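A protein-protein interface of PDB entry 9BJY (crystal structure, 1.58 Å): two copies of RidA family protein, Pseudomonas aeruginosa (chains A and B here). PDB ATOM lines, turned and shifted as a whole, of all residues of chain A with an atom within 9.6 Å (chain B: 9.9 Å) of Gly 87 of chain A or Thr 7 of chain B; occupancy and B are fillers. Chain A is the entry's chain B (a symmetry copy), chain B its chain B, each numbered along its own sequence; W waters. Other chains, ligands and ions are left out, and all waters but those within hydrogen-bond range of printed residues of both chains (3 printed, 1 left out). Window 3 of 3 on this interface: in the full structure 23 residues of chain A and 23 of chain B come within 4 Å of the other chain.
Of chain B, only Thr 7 comes within 4 Å of Gly 87 of chain A. Thr 7 of chain B touches one residue of chain A. No residue of chain B comes within 4 Å of Thr 86 of chain A. Gln 88 of chain A touches just one residue of chain B: Arg 4. Ala 89 of chain A touches just these residues of chain B: Arg 4, Asn 8, Arg 10, Leu 11 and Ser 12. No residue of chain A comes within 4 Å of Ala 6 of chain B. Of the printed residues of chain B, Ser 91 of chain A touches Ser 12, Val 15 and Ser 24. Of the printed residues of chain A, Asp 9 of chain B touches Thr 81 and Leu 84. Of the printed residues of chain A, Arg 10 of chain B touches Thr 81 (3.6 Å) and Ala 89 (3.8 Å). Printed residues of chain A within 4 Å of Ser 24 of chain B: Ser 91 (3.3 Å). Printed residues of chain B within 4 Å of Glu 57 of chain A: Arg 4. Ala 13 of chain B touches none of the printed residues of chain A.
Water W2 bridges the side-chain amide nitrogen of Gln 88 of chain A (2.4 Å) and the guanidinium group of Arg 4 of chain B (2.4 Å). Water W3 lies within hydrogen-bond range of the backbone carbonyl oxygen of Asp 9 of chain B (2.6 Å) and the backbone carbonyl oxygen of Thr 81 of chain A (2.7 Å). Water W1 lies within hydrogen-bond range of O of Asn 8 of chain B (2.7 Å), N of Ala 89 of chain A (3.0 Å) and N of Gln 88 of chain A (3.1 Å).
NH2 of Arg 4 of chain B is in hydrogen-bond range of O of Glu 57 of chain A (2.8 Å). The backbone carbonyl oxygen (O) of Gln 88 of chain A is in hydrogen-bond range of the guanidinium group (NE) of Arg 4 of chain B (3.5 Å). O of Ala 89 of chain A lies close to NE of Arg 4 of chain B (3.3 Å). OG of Ser 12 of chain B sits at hydrogen-bond distance from O of Ala 89 of chain A (2.7 Å). The backbone NH (N) of Ser 12 of chain B lies within hydrogen-bond range of the backbone carbonyl oxygen (O) of Pro 90 of chain A (2.9 Å).
No position is printed for both chains.
Among the printed residues, pairs that only touch across the chains: Thr 81 of chain A with Asp 9 of chain B (3.3 Å), Thr 81 of chain A with Arg 10 of chain B (3.6 Å), Leu 84 of chain A with Asp 9 of chain B (3.99 Å), Gly 87 of chain A with Thr 7 of chain B (3.7 Å), Ala 89 of chain A with Asn 8 of chain B (3.5 Å), Ala 89 of chain A with Arg 10 of chain B (3.8 Å), Ala 89 of chain A with Leu 11 of chain B (3.5 Å), Pro 90 of chain A with Leu 11 of chain B (3.4 Å), Pro 90 of chain A with Val 15 of chain B (3.9 Å), Ser 91 of chain A with Ser 12 of chain B (3.4 Å), Ser 91 of chain A with Val 15 of chain B (3.4 Å) and Ser 91 of chain A with Ser 24 of chain B (3.3 Å).
Of the 14 printed residues of chain A, 8 touch a printed residue of chain B. Of the 18 printed residues of chain B, 9 touch a printed residue of chain A. Along chain B the printed residues that touch a printed residue of chain A span positions 4 to 24. Among the printed residues, no Asp or Glu carboxylate lies within 4 Å of a Lys or Arg side-chain nitrogen of the other chain.
OG of Ser 12 of chain B sits at hydrogen-bond distance from OG1 of Thr 7 of chain B, at 2.7 Å. The side-chain amide oxygen (OD1) of Asn 8 of chain B is in hydrogen-bond range of the backbone NH (N) of Arg 10 of chain B, 2.8 Å away. The side-chain amide oxygen (OD1) of Asn 8 of chain B is in hydrogen-bond range of the backbone NH (N) of Leu 11 of chain B. The backbone carbonyl oxygen (O) of Ser 12 of chain B lies within hydrogen-bond range of the side-chain hydroxyl (OG) of Ser 24 of chain B, 2.7 Å away. The backbone NH of Ser 24 of chain B lies within hydrogen-bond range of the backbone carbonyl oxygen of Ala 13 of chain B, 2.9 Å away. The backbone carbonyl oxygen of Thr 86 of chain A sits close to the side-chain amide oxygen of Gln 88 of chain A, at 3.4 Å.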
ATOM      1  N   LYS A  56      -7.067 -20.040  22.019  1.00  0.00           N
ATOM      2  CA  LYS A  56      -5.665 -20.382  22.190  1.00  0.00           C
ATOM      3  C   LYS A  56      -5.172 -20.003  23.575  1.00  0.00           C
ATOM      4  O   LYS A  56      -4.325 -20.707  24.142  1.00  0.00           O
ATOM      5  CB  LYS A  56      -4.849 -19.653  21.114  1.00  0.00           C
ATOM      6  CG  LYS A  56      -5.288 -19.983  19.688  1.00  0.00           C
ATOM      7  CD  LYS A  56      -4.731 -18.926  18.727  1.00  0.00           C
ATOM      8  CE  LYS A  56      -5.007 -19.214  17.277  1.00  0.00           C
ATOM      9  NZ  LYS A  56      -3.990 -18.557  16.375  1.00  0.00           N
ATOM     10  N   GLU A  57      -5.706 -18.913  24.136  1.00  0.00           N
ATOM     11  CA  GLU A  57      -5.295 -18.422  25.452  1.00  0.00           C
ATOM     12  C   GLU A  57      -5.731 -19.330  26.590  1.00  0.00           C
ATOM     13  O   GLU A  57      -5.320 -19.103  27.739  1.00  0.00           O
ATOM     14  CB  GLU A  57      -5.855 -17.008  25.666  1.00  0.00           C
ATOM     15  CG  GLU A  57      -5.274 -15.953  24.702  1.00  0.00           C
ATOM     16  CD  GLU A  57      -5.993 -15.843  23.357  1.00  0.00           C
ATOM     17  OE1 GLU A  57      -6.890 -16.663  23.052  1.00  0.00           O
ATOM     18  OE2 GLU A  57      -5.620 -14.931  22.581  1.00  0.00           O
ATOM     19  N   ILE A  59      -5.537 -22.887  26.454  1.00  0.00           N
ATOM     20  CA  ILE A  59      -4.987 -24.234  26.371  1.00  0.00           C
ATOM     21  C   ILE A  59      -4.393 -24.608  27.721  1.00  0.00           C
ATOM     22  O   ILE A  59      -3.687 -23.806  28.358  1.00  0.00           O
ATOM     23  CB  ILE A  59      -3.960 -24.342  25.228  1.00  0.00           C
ATOM     24  CG1 ILE A  59      -4.652 -24.041  23.901  1.00  0.00           C
ATOM     25  CG2 ILE A  59      -3.340 -25.750  25.217  1.00  0.00           C
ATOM     26  CD1 ILE A  59      -3.722 -23.847  22.685  1.00  0.00           C
ATOM     27  N   THR A  81       6.501 -21.016  19.369  1.00  0.00           N
ATOM     28  CA  THR A  81       6.667 -19.846  20.220  1.00  0.00           C
ATOM     29  C   THR A  81       6.059 -18.612  19.575  1.00  0.00           C
ATOM     30  O   THR A  81       5.538 -17.744  20.278  1.00  0.00           O
ATOM     31  CB  THR A  81       8.142 -19.588  20.509  1.00  0.00           C
ATOM     32  OG1 THR A  81       8.852 -19.422  19.279  1.00  0.00           O
ATOM     33  CG2 THR A  81       8.740 -20.732  21.289  1.00  0.00           C
ATOM     34  N   GLN A  82       6.103 -18.526  18.247  1.00  0.00           N
ATOM     35  CA  GLN A  82       5.517 -17.366  17.579  1.00  0.00           C
ATOM     36  C   GLN A  82       4.000 -17.412  17.589  1.00  0.00           C
ATOM     37  O   GLN A  82       3.347 -16.361  17.571  1.00  0.00           O
ATOM     38  CB  GLN A  82       6.017 -17.309  16.136  1.00  0.00           C
ATOM     39  CG  GLN A  82       5.415 -16.201  15.281  1.00  0.00           C
ATOM     40  CD  GLN A  82       5.705 -14.820  15.840  1.00  0.00           C
ATOM     41  OE1 GLN A  82       6.703 -14.616  16.545  1.00  0.00           O
ATOM     42  NE2 GLN A  82       4.826 -13.863  15.544  1.00  0.00           N
ATOM     43  N   TRP A  83       3.420 -18.608  17.650  1.00  0.00           N
ATOM     44  CA  TRP A  83       1.971 -18.769  17.576  1.00  0.00           C
ATOM     45  C   TRP A  83       1.283 -18.528  18.903  1.00  0.00           C
ATOM     46  O   TRP A  83       0.137 -18.056  18.935  1.00  0.00           O
ATOM     47  CB  TRP A  83       1.648 -20.184  17.118  1.00  0.00           C
ATOM     48  CG  TRP A  83       0.211 -20.573  17.018  1.00  0.00           C
ATOM     49  CD1 TRP A  83      -0.625 -20.289  16.001  1.00  0.00           C
ATOM     50  CD2 TRP A  83      -0.539 -21.392  17.939  1.00  0.00           C
ATOM     51  NE1 TRP A  83      -1.860 -20.864  16.218  1.00  0.00           N
ATOM     52  CE2 TRP A  83      -1.838 -21.529  17.413  1.00  0.00           C
ATOM     53  CE3 TRP A  83      -0.245 -21.990  19.166  1.00  0.00           C
ATOM     54  CZ2 TRP A  83      -2.846 -22.259  18.064  1.00  0.00           C
ATOM     55  CZ3 TRP A  83      -1.246 -22.714  19.813  1.00  0.00           C
ATOM     56  CH2 TRP A  83      -2.526 -22.845  19.259  1.00  0.00           C
ATOM     57  N   LEU A  84       1.943 -18.865  19.998  1.00  0.00           N
ATOM     58  CA  LEU A  84       1.270 -18.826  21.281  1.00  0.00           C
ATOM     59  C   LEU A  84       0.899 -17.395  21.631  1.00  0.00           C
ATOM     60  O   LEU A  84       1.695 -16.472  21.407  1.00  0.00           O
ATOM     61  CB  LEU A  84       2.170 -19.413  22.363  1.00  0.00           C
ATOM     62  CG  LEU A  84       2.294 -20.939  22.327  1.00  0.00           C
ATOM     63  CD1 LEU A  84       3.334 -21.343  23.338  1.00  0.00           C
ATOM     64  CD2 LEU A  84       0.962 -21.538  22.644  1.00  0.00           C
ATOM     65  N   PRO A  85      -0.271 -17.179  22.227  1.00  0.00           N
ATOM     66  CA  PRO A  85      -0.575 -15.851  22.746  1.00  0.00           C
ATOM     67  C   PRO A  85       0.446 -15.466  23.799  1.00  0.00           C
ATOM     68  O   PRO A  85       0.851 -16.280  24.642  1.00  0.00           O
ATOM     69  CB  PRO A  85      -1.980 -16.013  23.332  1.00  0.00           C
ATOM     70  CG  PRO A  85      -2.615 -17.069  22.426  1.00  0.00           C
ATOM     71  CD  PRO A  85      -1.470 -18.048  22.187  1.00  0.00           C
ATOM     72  N   THR A  86       0.861 -14.203  23.742  1.00  0.00           N
ATOM     73  CA  THR A  86       1.969 -13.727  24.551  1.00  0.00           C
ATOM     74  C   THR A  86       1.732 -13.971  26.036  1.00  0.00           C
ATOM     75  O   THR A  86       0.667 -13.646  26.579  1.00  0.00           O
ATOM     76  CB  THR A  86       2.176 -12.233  24.268  1.00  0.00           C
ATOM     77  OG1 THR A  86       2.349 -12.024  22.850  1.00  0.00           O
ATOM     78  CG2 THR A  86       3.391 -11.706  24.996  1.00  0.00           C
ATOM     79  N   GLY A  87       2.741 -14.555  26.692  1.00  0.00           N
ATOM     80  CA  GLY A  87       2.711 -14.825  28.116  1.00  0.00           C
ATOM     81  C   GLY A  87       1.746 -15.897  28.561  1.00  0.00           C
ATOM     82  O   GLY A  87       1.520 -16.050  29.773  1.00  0.00           O
ATOM     83  N   GLN A  88       1.172 -16.655  27.641  1.00  0.00           N
ATOM     84  CA  GLN A  88       0.103 -17.590  27.963  1.00  0.00           C
ATOM     85  C   GLN A  88       0.404 -18.992  27.435  1.00  0.00           C
ATOM     86  O   GLN A  88      -0.496 -19.724  27.022  1.00  0.00           O
ATOM     87  CB  GLN A  88      -1.230 -17.075  27.419  1.00  0.00           C
ATOM     88  CG  GLN A  88      -1.581 -15.711  28.039  1.00  0.00           C
ATOM     89  CD  GLN A  88      -2.754 -15.026  27.381  1.00  0.00           C
ATOM     90  OE1 GLN A  88      -2.641 -14.462  26.294  1.00  0.00           O
ATOM     91  NE2 GLN A  88      -3.882 -15.031  28.069  1.00  0.00           N
ATOM     92  N   ALA A  89       1.664 -19.402  27.485  1.00  0.00           N
ATOM     93  CA  ALA A  89       1.993 -20.756  27.048  1.00  0.00           C
ATOM     94  C   ALA A  89       1.328 -21.782  27.935  1.00  0.00           C
ATOM     95  O   ALA A  89       1.257 -21.597  29.171  1.00  0.00           O
ATOM     96  CB  ALA A  89       3.505 -20.977  27.055  1.00  0.00           C
ATOM     97  N   PRO A  90       0.874 -22.911  27.394  1.00  0.00           N
ATOM     98  CA  PRO A  90       0.285 -23.983  28.184  1.00  0.00           C
ATOM     99  C   PRO A  90       1.364 -24.906  28.750  1.00  0.00           C
ATOM    100  O   PRO A  90       2.554 -24.758  28.481  1.00  0.00           O
ATOM    101  CB  PRO A  90      -0.577 -24.722  27.159  1.00  0.00           C
ATOM    102  CG  PRO A  90       0.270 -24.645  25.914  1.00  0.00           C
ATOM    103  CD  PRO A  90       0.826 -23.225  25.939  1.00  0.00           C
ATOM    104  N   SER A  91       0.938 -25.879  29.548  1.00  0.00           N
ATOM    105  CA  SER A  91       1.847 -26.986  29.832  1.00  0.00           C
ATOM    106  C   SER A  91       2.073 -27.773  28.544  1.00  0.00           C
ATOM    107  O   SER A  91       1.195 -27.853  27.678  1.00  0.00           O
ATOM    108  CB  SER A  91       1.310 -27.871  30.947  1.00  0.00           C
ATOM    109  OG  SER A  91       0.204 -28.671  30.561  1.00  0.00           O
ATOM    110  N   PRO B   2      -7.711 -20.011  33.697  1.00  0.00           N
ATOM    111  CA  PRO B   2      -6.493 -20.758  34.026  1.00  0.00           C
ATOM    112  C   PRO B   2      -5.491 -19.897  34.770  1.00  0.00           C
ATOM    113  O   PRO B   2      -5.389 -18.687  34.557  1.00  0.00           O
ATOM    114  CB  PRO B   2      -5.949 -21.190  32.660  1.00  0.00           C
ATOM    115  CG  PRO B   2      -7.078 -21.081  31.716  1.00  0.00           C
ATOM    116  CD  PRO B   2      -7.971 -19.996  32.242  1.00  0.00           C
ATOM    117  N   THR B   3      -4.738 -20.539  35.653  1.00  0.00           N
ATOM    118  CA  THR B   3      -3.607 -19.902  36.302  1.00  0.00           C
ATOM    119  C   THR B   3      -2.353 -20.623  35.843  1.00  0.00           C
ATOM    120  O   THR B   3      -2.387 -21.830  35.601  1.00  0.00           O
ATOM    121  CB  THR B   3      -3.686 -20.006  37.826  1.00  0.00           C
ATOM    122  OG1 THR B   3      -4.914 -19.431  38.275  1.00  0.00           O
ATOM    123  CG2 THR B   3      -2.518 -19.253  38.455  1.00  0.00           C
ATOM    124  N   ARG B   4      -1.242 -19.898  35.739  1.00  0.00           N
ATOM    125  CA  ARG B   4      -0.034 -20.482  35.189  1.00  0.00           C
ATOM    126  C   ARG B   4       1.111 -20.333  36.180  1.00  0.00           C
ATOM    127  O   ARG B   4       1.171 -19.370  36.956  1.00  0.00           O
ATOM    128  CB  ARG B   4       0.370 -19.881  33.850  1.00  0.00           C
ATOM    129  CG  ARG B   4      -0.711 -19.958  32.801  1.00  0.00           C
ATOM    130  CD  ARG B   4      -0.153 -19.834  31.388  1.00  0.00           C
ATOM    131  NE  ARG B   4      -1.226 -19.777  30.401  1.00  0.00           N
ATOM    132  CZ  ARG B   4      -2.108 -18.792  30.363  1.00  0.00           C
ATOM    133  NH1 ARG B   4      -1.988 -17.733  31.147  1.00  0.00           N
ATOM    134  NH2 ARG B   4      -3.125 -18.858  29.511  1.00  0.00           N
ATOM    135  N   ILE B   5       2.006 -21.312  36.159  1.00  0.00           N
ATOM    136  CA  ILE B   5       3.176 -21.340  37.032  1.00  0.00           C
ATOM    137  C   ILE B   5       4.432 -21.472  36.188  1.00  0.00           C
ATOM    138  O   ILE B   5       4.517 -22.352  35.321  1.00  0.00           O
ATOM    139  CB  ILE B   5       3.070 -22.489  38.046  1.00  0.00           C
ATOM    140  CG1 ILE B   5       1.854 -22.222  38.918  1.00  0.00           C
ATOM    141  CG2 ILE B   5       4.345 -22.582  38.849  1.00  0.00           C
ATOM    142  CD1 ILE B   5       1.273 -23.437  39.490  1.00  0.00           C
ATOM    143  N   ALA B   6       5.383 -20.564  36.413  1.00  0.00           N
ATOM    144  CA  ALA B   6       6.704 -20.575  35.785  1.00  0.00           C
ATOM    145  C   ALA B   6       6.560 -20.642  34.275  1.00  0.00           C
ATOM    146  O   ALA B   6       6.808 -21.689  33.665  1.00  0.00           O
ATOM    147  CB  ALA B   6       7.561 -21.724  36.301  1.00  0.00           C
ATOM    148  N   THR B   7       6.183 -19.515  33.680  1.00  0.00           N
ATOM    149  CA  THR B   7       5.878 -19.403  32.266  1.00  0.00           C
ATOM    150  C   THR B   7       7.052 -18.789  31.524  1.00  0.00           C
ATOM    151  O   THR B   7       7.687 -17.846  32.011  1.00  0.00           O
ATOM    152  CB  THR B   7       4.635 -18.532  32.049  1.00  0.00           C
ATOM    153  OG1 THR B   7       3.525 -19.080  32.787  1.00  0.00           O
ATOM    154  CG2 THR B   7       4.293 -18.424  30.567  1.00  0.00           C
ATOM    155  N   ASN B   8       7.352 -19.338  30.349  1.00  0.00           N
ATOM    156  CA  ASN B   8       8.236 -18.687  29.395  1.00  0.00           C
ATOM    157  C   ASN B   8       7.573 -18.798  28.027  1.00  0.00           C
ATOM    158  O   ASN B   8       6.410 -19.181  27.922  1.00  0.00           O
ATOM    159  CB  ASN B   8       9.653 -19.268  29.422  1.00  0.00           C
ATOM    160  CG  ASN B   8       9.713 -20.733  29.033  1.00  0.00           C
ATOM    161  OD1 ASN B   8       8.931 -21.230  28.208  1.00  0.00           O
ATOM    162  ND2 ASN B   8      10.673 -21.437  29.616  1.00  0.00           N
ATOM    163  N   ASP B   9       8.312 -18.467  26.967  1.00  0.00           N
ATOM    164  CA  ASP B   9       7.665 -18.387  25.666  1.00  0.00           C
ATOM    165  C   ASP B   9       7.485 -19.750  25.008  1.00  0.00           C
ATOM    166  O   ASP B   9       6.975 -19.813  23.889  1.00  0.00           O
ATOM    167  CB  ASP B   9       8.428 -17.442  24.734  1.00  0.00           C
ATOM    168  CG  ASP B   9       9.857 -17.856  24.486  1.00  0.00           C
ATOM    169  OD1 ASP B   9      10.284 -18.962  24.901  1.00  0.00           O
ATOM    170  OD2 ASP B   9      10.580 -17.048  23.859  1.00  0.00           O
ATOM    171  N   ARG B  10       7.899 -20.829  25.670  1.00  0.00           N
ATOM    172  CA  ARG B  10       7.675 -22.185  25.178  1.00  0.00           C
ATOM    173  C   ARG B  10       6.634 -22.944  25.983  1.00  0.00           C
ATOM    174  O   ARG B  10       5.877 -23.726  25.420  1.00  0.00           O
ATOM    175  CB  ARG B  10       8.990 -22.981  25.176  1.00  0.00           C
ATOM    176  CG  ARG B  10      10.019 -22.426  24.181  1.00  0.00           C
ATOM    177  CD  ARG B  10      11.445 -22.600  24.666  1.00  0.00           C
ATOM    178  NE  ARG B  10      11.934 -23.972  24.543  1.00  0.00           N
ATOM    179  CZ  ARG B  10      12.656 -24.434  23.527  1.00  0.00           C
ATOM    180  NH1 ARG B  10      12.948 -23.677  22.481  1.00  0.00           N
ATOM    181  NH2 ARG B  10      13.092 -25.692  23.563  1.00  0.00           N
ATOM    182  N   LEU B  11       6.586 -22.753  27.299  1.00  0.00           N
ATOM    183  CA  LEU B  11       5.682 -23.542  28.121  1.00  0.00           C
ATOM    184  C   LEU B  11       5.512 -22.875  29.475  1.00  0.00           C
ATOM    185  O   LEU B  11       6.323 -22.036  29.882  1.00  0.00           O
ATOM    186  CB  LEU B  11       6.221 -24.975  28.295  1.00  0.00           C
ATOM    187  CG  LEU B  11       7.393 -25.225  29.251  1.00  0.00           C
ATOM    188  CD1 LEU B  11       7.782 -26.739  29.289  1.00  0.00           C
ATOM    189  CD2 LEU B  11       8.581 -24.360  28.905  1.00  0.00           C
ATOM    190  N   SER B  12       4.451 -23.270  30.168  1.00  0.00           N
ATOM    191  CA  SER B  12       4.335 -23.046  31.598  1.00  0.00           C
ATOM    192  C   SER B  12       4.630 -24.365  32.288  1.00  0.00           C
ATOM    193  O   SER B  12       4.153 -25.416  31.846  1.00  0.00           O
ATOM    194  CB  SER B  12       2.943 -22.551  31.988  1.00  0.00           C
ATOM    195  OG  SER B  12       2.637 -21.274  31.450  1.00  0.00           O
ATOM    196  N   ALA B  13       5.407 -24.326  33.373  1.00  0.00           N
ATOM    197  CA  ALA B  13       5.681 -25.578  34.082  1.00  0.00           C
ATOM    198  C   ALA B  13       4.392 -26.237  34.562  1.00  0.00           C
ATOM    199  O   ALA B  13       4.283 -27.473  34.584  1.00  0.00           O
ATOM    200  CB  ALA B  13       6.606 -25.330  35.283  1.00  0.00           C
ATOM    201  N   ALA B  14       3.416 -25.444  34.979  1.00  0.00           N
ATOM    202  CA  ALA B  14       2.102 -25.948  35.336  1.00  0.00           C
ATOM    203  C   ALA B  14       1.016 -24.969  34.909  1.00  0.00           C
ATOM    204  O   ALA B  14       1.219 -23.748  34.895  1.00  0.00           O
ATOM    205  CB  ALA B  14       1.994 -26.204  36.841  1.00  0.00           C
ATOM    206  N   VAL B  15      -0.149 -25.525  34.563  1.00  0.00           N
ATOM    207  CA  VAL B  15      -1.370 -24.756  34.361  1.00  0.00           C
ATOM    208  C   VAL B  15      -2.439 -25.339  35.279  1.00  0.00           C
ATOM    209  O   VAL B  15      -2.635 -26.562  35.310  1.00  0.00           O
ATOM    210  CB  VAL B  15      -1.827 -24.779  32.894  1.00  0.00           C
ATOM    211  CG1 VAL B  15      -3.110 -23.978  32.746  1.00  0.00           C
ATOM    212  CG2 VAL B  15      -0.761 -24.204  31.980  1.00  0.00           C
ATOM    213  N   CYS B  16      -3.105 -24.475  36.039  1.00  0.00           N
ATOM    214  CA  CYS B  16      -4.143 -24.853  36.981  1.00  0.00           C
ATOM    215  C   CYS B  16      -5.485 -24.378  36.451  1.00  0.00           C
ATOM    216  O   CYS B  16      -5.587 -23.254  35.947  1.00  0.00           O
ATOM    217  CB  CYS B  16      -3.880 -24.239  38.349  1.00  0.00           C
ATOM    218  SG  CYS B  16      -2.201 -24.630  38.969  1.00  0.00           S
ATOM    219  N   SER B  24       3.801 -29.714  32.867  1.00  0.00           N
ATOM    220  CA  SER B  24       4.653 -30.020  31.724  1.00  0.00           C
ATOM    221  C   SER B  24       5.467 -31.273  32.013  1.00  0.00           C
ATOM    222  O   SER B  24       5.768 -31.592  33.162  1.00  0.00           O
ATOM    223  CB  SER B  24       5.584 -28.843  31.436  1.00  0.00           C
ATOM    224  OG  SER B  24       4.888 -27.780  30.811  1.00  0.00           O
ATOM    225  N   LEU B  48       7.015 -29.008  41.800  1.00  0.00           N
ATOM    226  CA  LEU B  48       5.983 -28.328  41.022  1.00  0.00           C
ATOM    227  C   LEU B  48       4.581 -28.570  41.566  1.00  0.00           C
ATOM    228  O   LEU B  48       3.750 -27.663  41.537  1.00  0.00           O
ATOM    229  CB  LEU B  48       5.984 -28.752  39.557  1.00  0.00           C
ATOM    230  CG  LEU B  48       6.727 -27.975  38.492  1.00  0.00           C
ATOM    231  CD1 LEU B  48       6.529 -28.692  37.159  1.00  0.00           C
ATOM    232  CD2 LEU B  48       6.169 -26.574  38.459  1.00  0.00           C
ATOM    233  N   GLU B  51       4.110 -25.973  44.193  1.00  0.00           N
ATOM    234  CA  GLU B  51       3.846 -24.627  43.717  1.00  0.00           C
ATOM    235  C   GLU B  51       2.457 -24.493  43.109  1.00  0.00           C
ATOM    236  O   GLU B  51       1.850 -23.422  43.179  1.00  0.00           O
ATOM    237  CB  GLU B  51       4.884 -24.218  42.687  1.00  0.00           C
ATOM    238  CG  GLU B  51       4.864 -22.733  42.401  1.00  0.00           C
ATOM    239  CD  GLU B  51       5.420 -21.915  43.562  1.00  0.00           C
ATOM    240  OE1 GLU B  51       5.874 -22.524  44.555  1.00  0.00           O
ATOM    241  OE2 GLU B  51       5.404 -20.665  43.483  1.00  0.00           O
HETATM  242  O   HOH W   1       4.133 -17.718  27.484  1.00  0.00           O
HETATM  243  O   HOH W   2      -3.979 -16.608  29.928  1.00  0.00           O
HETATM  244  O   HOH W   3       5.647 -17.721  23.019  1.00  0.00           O
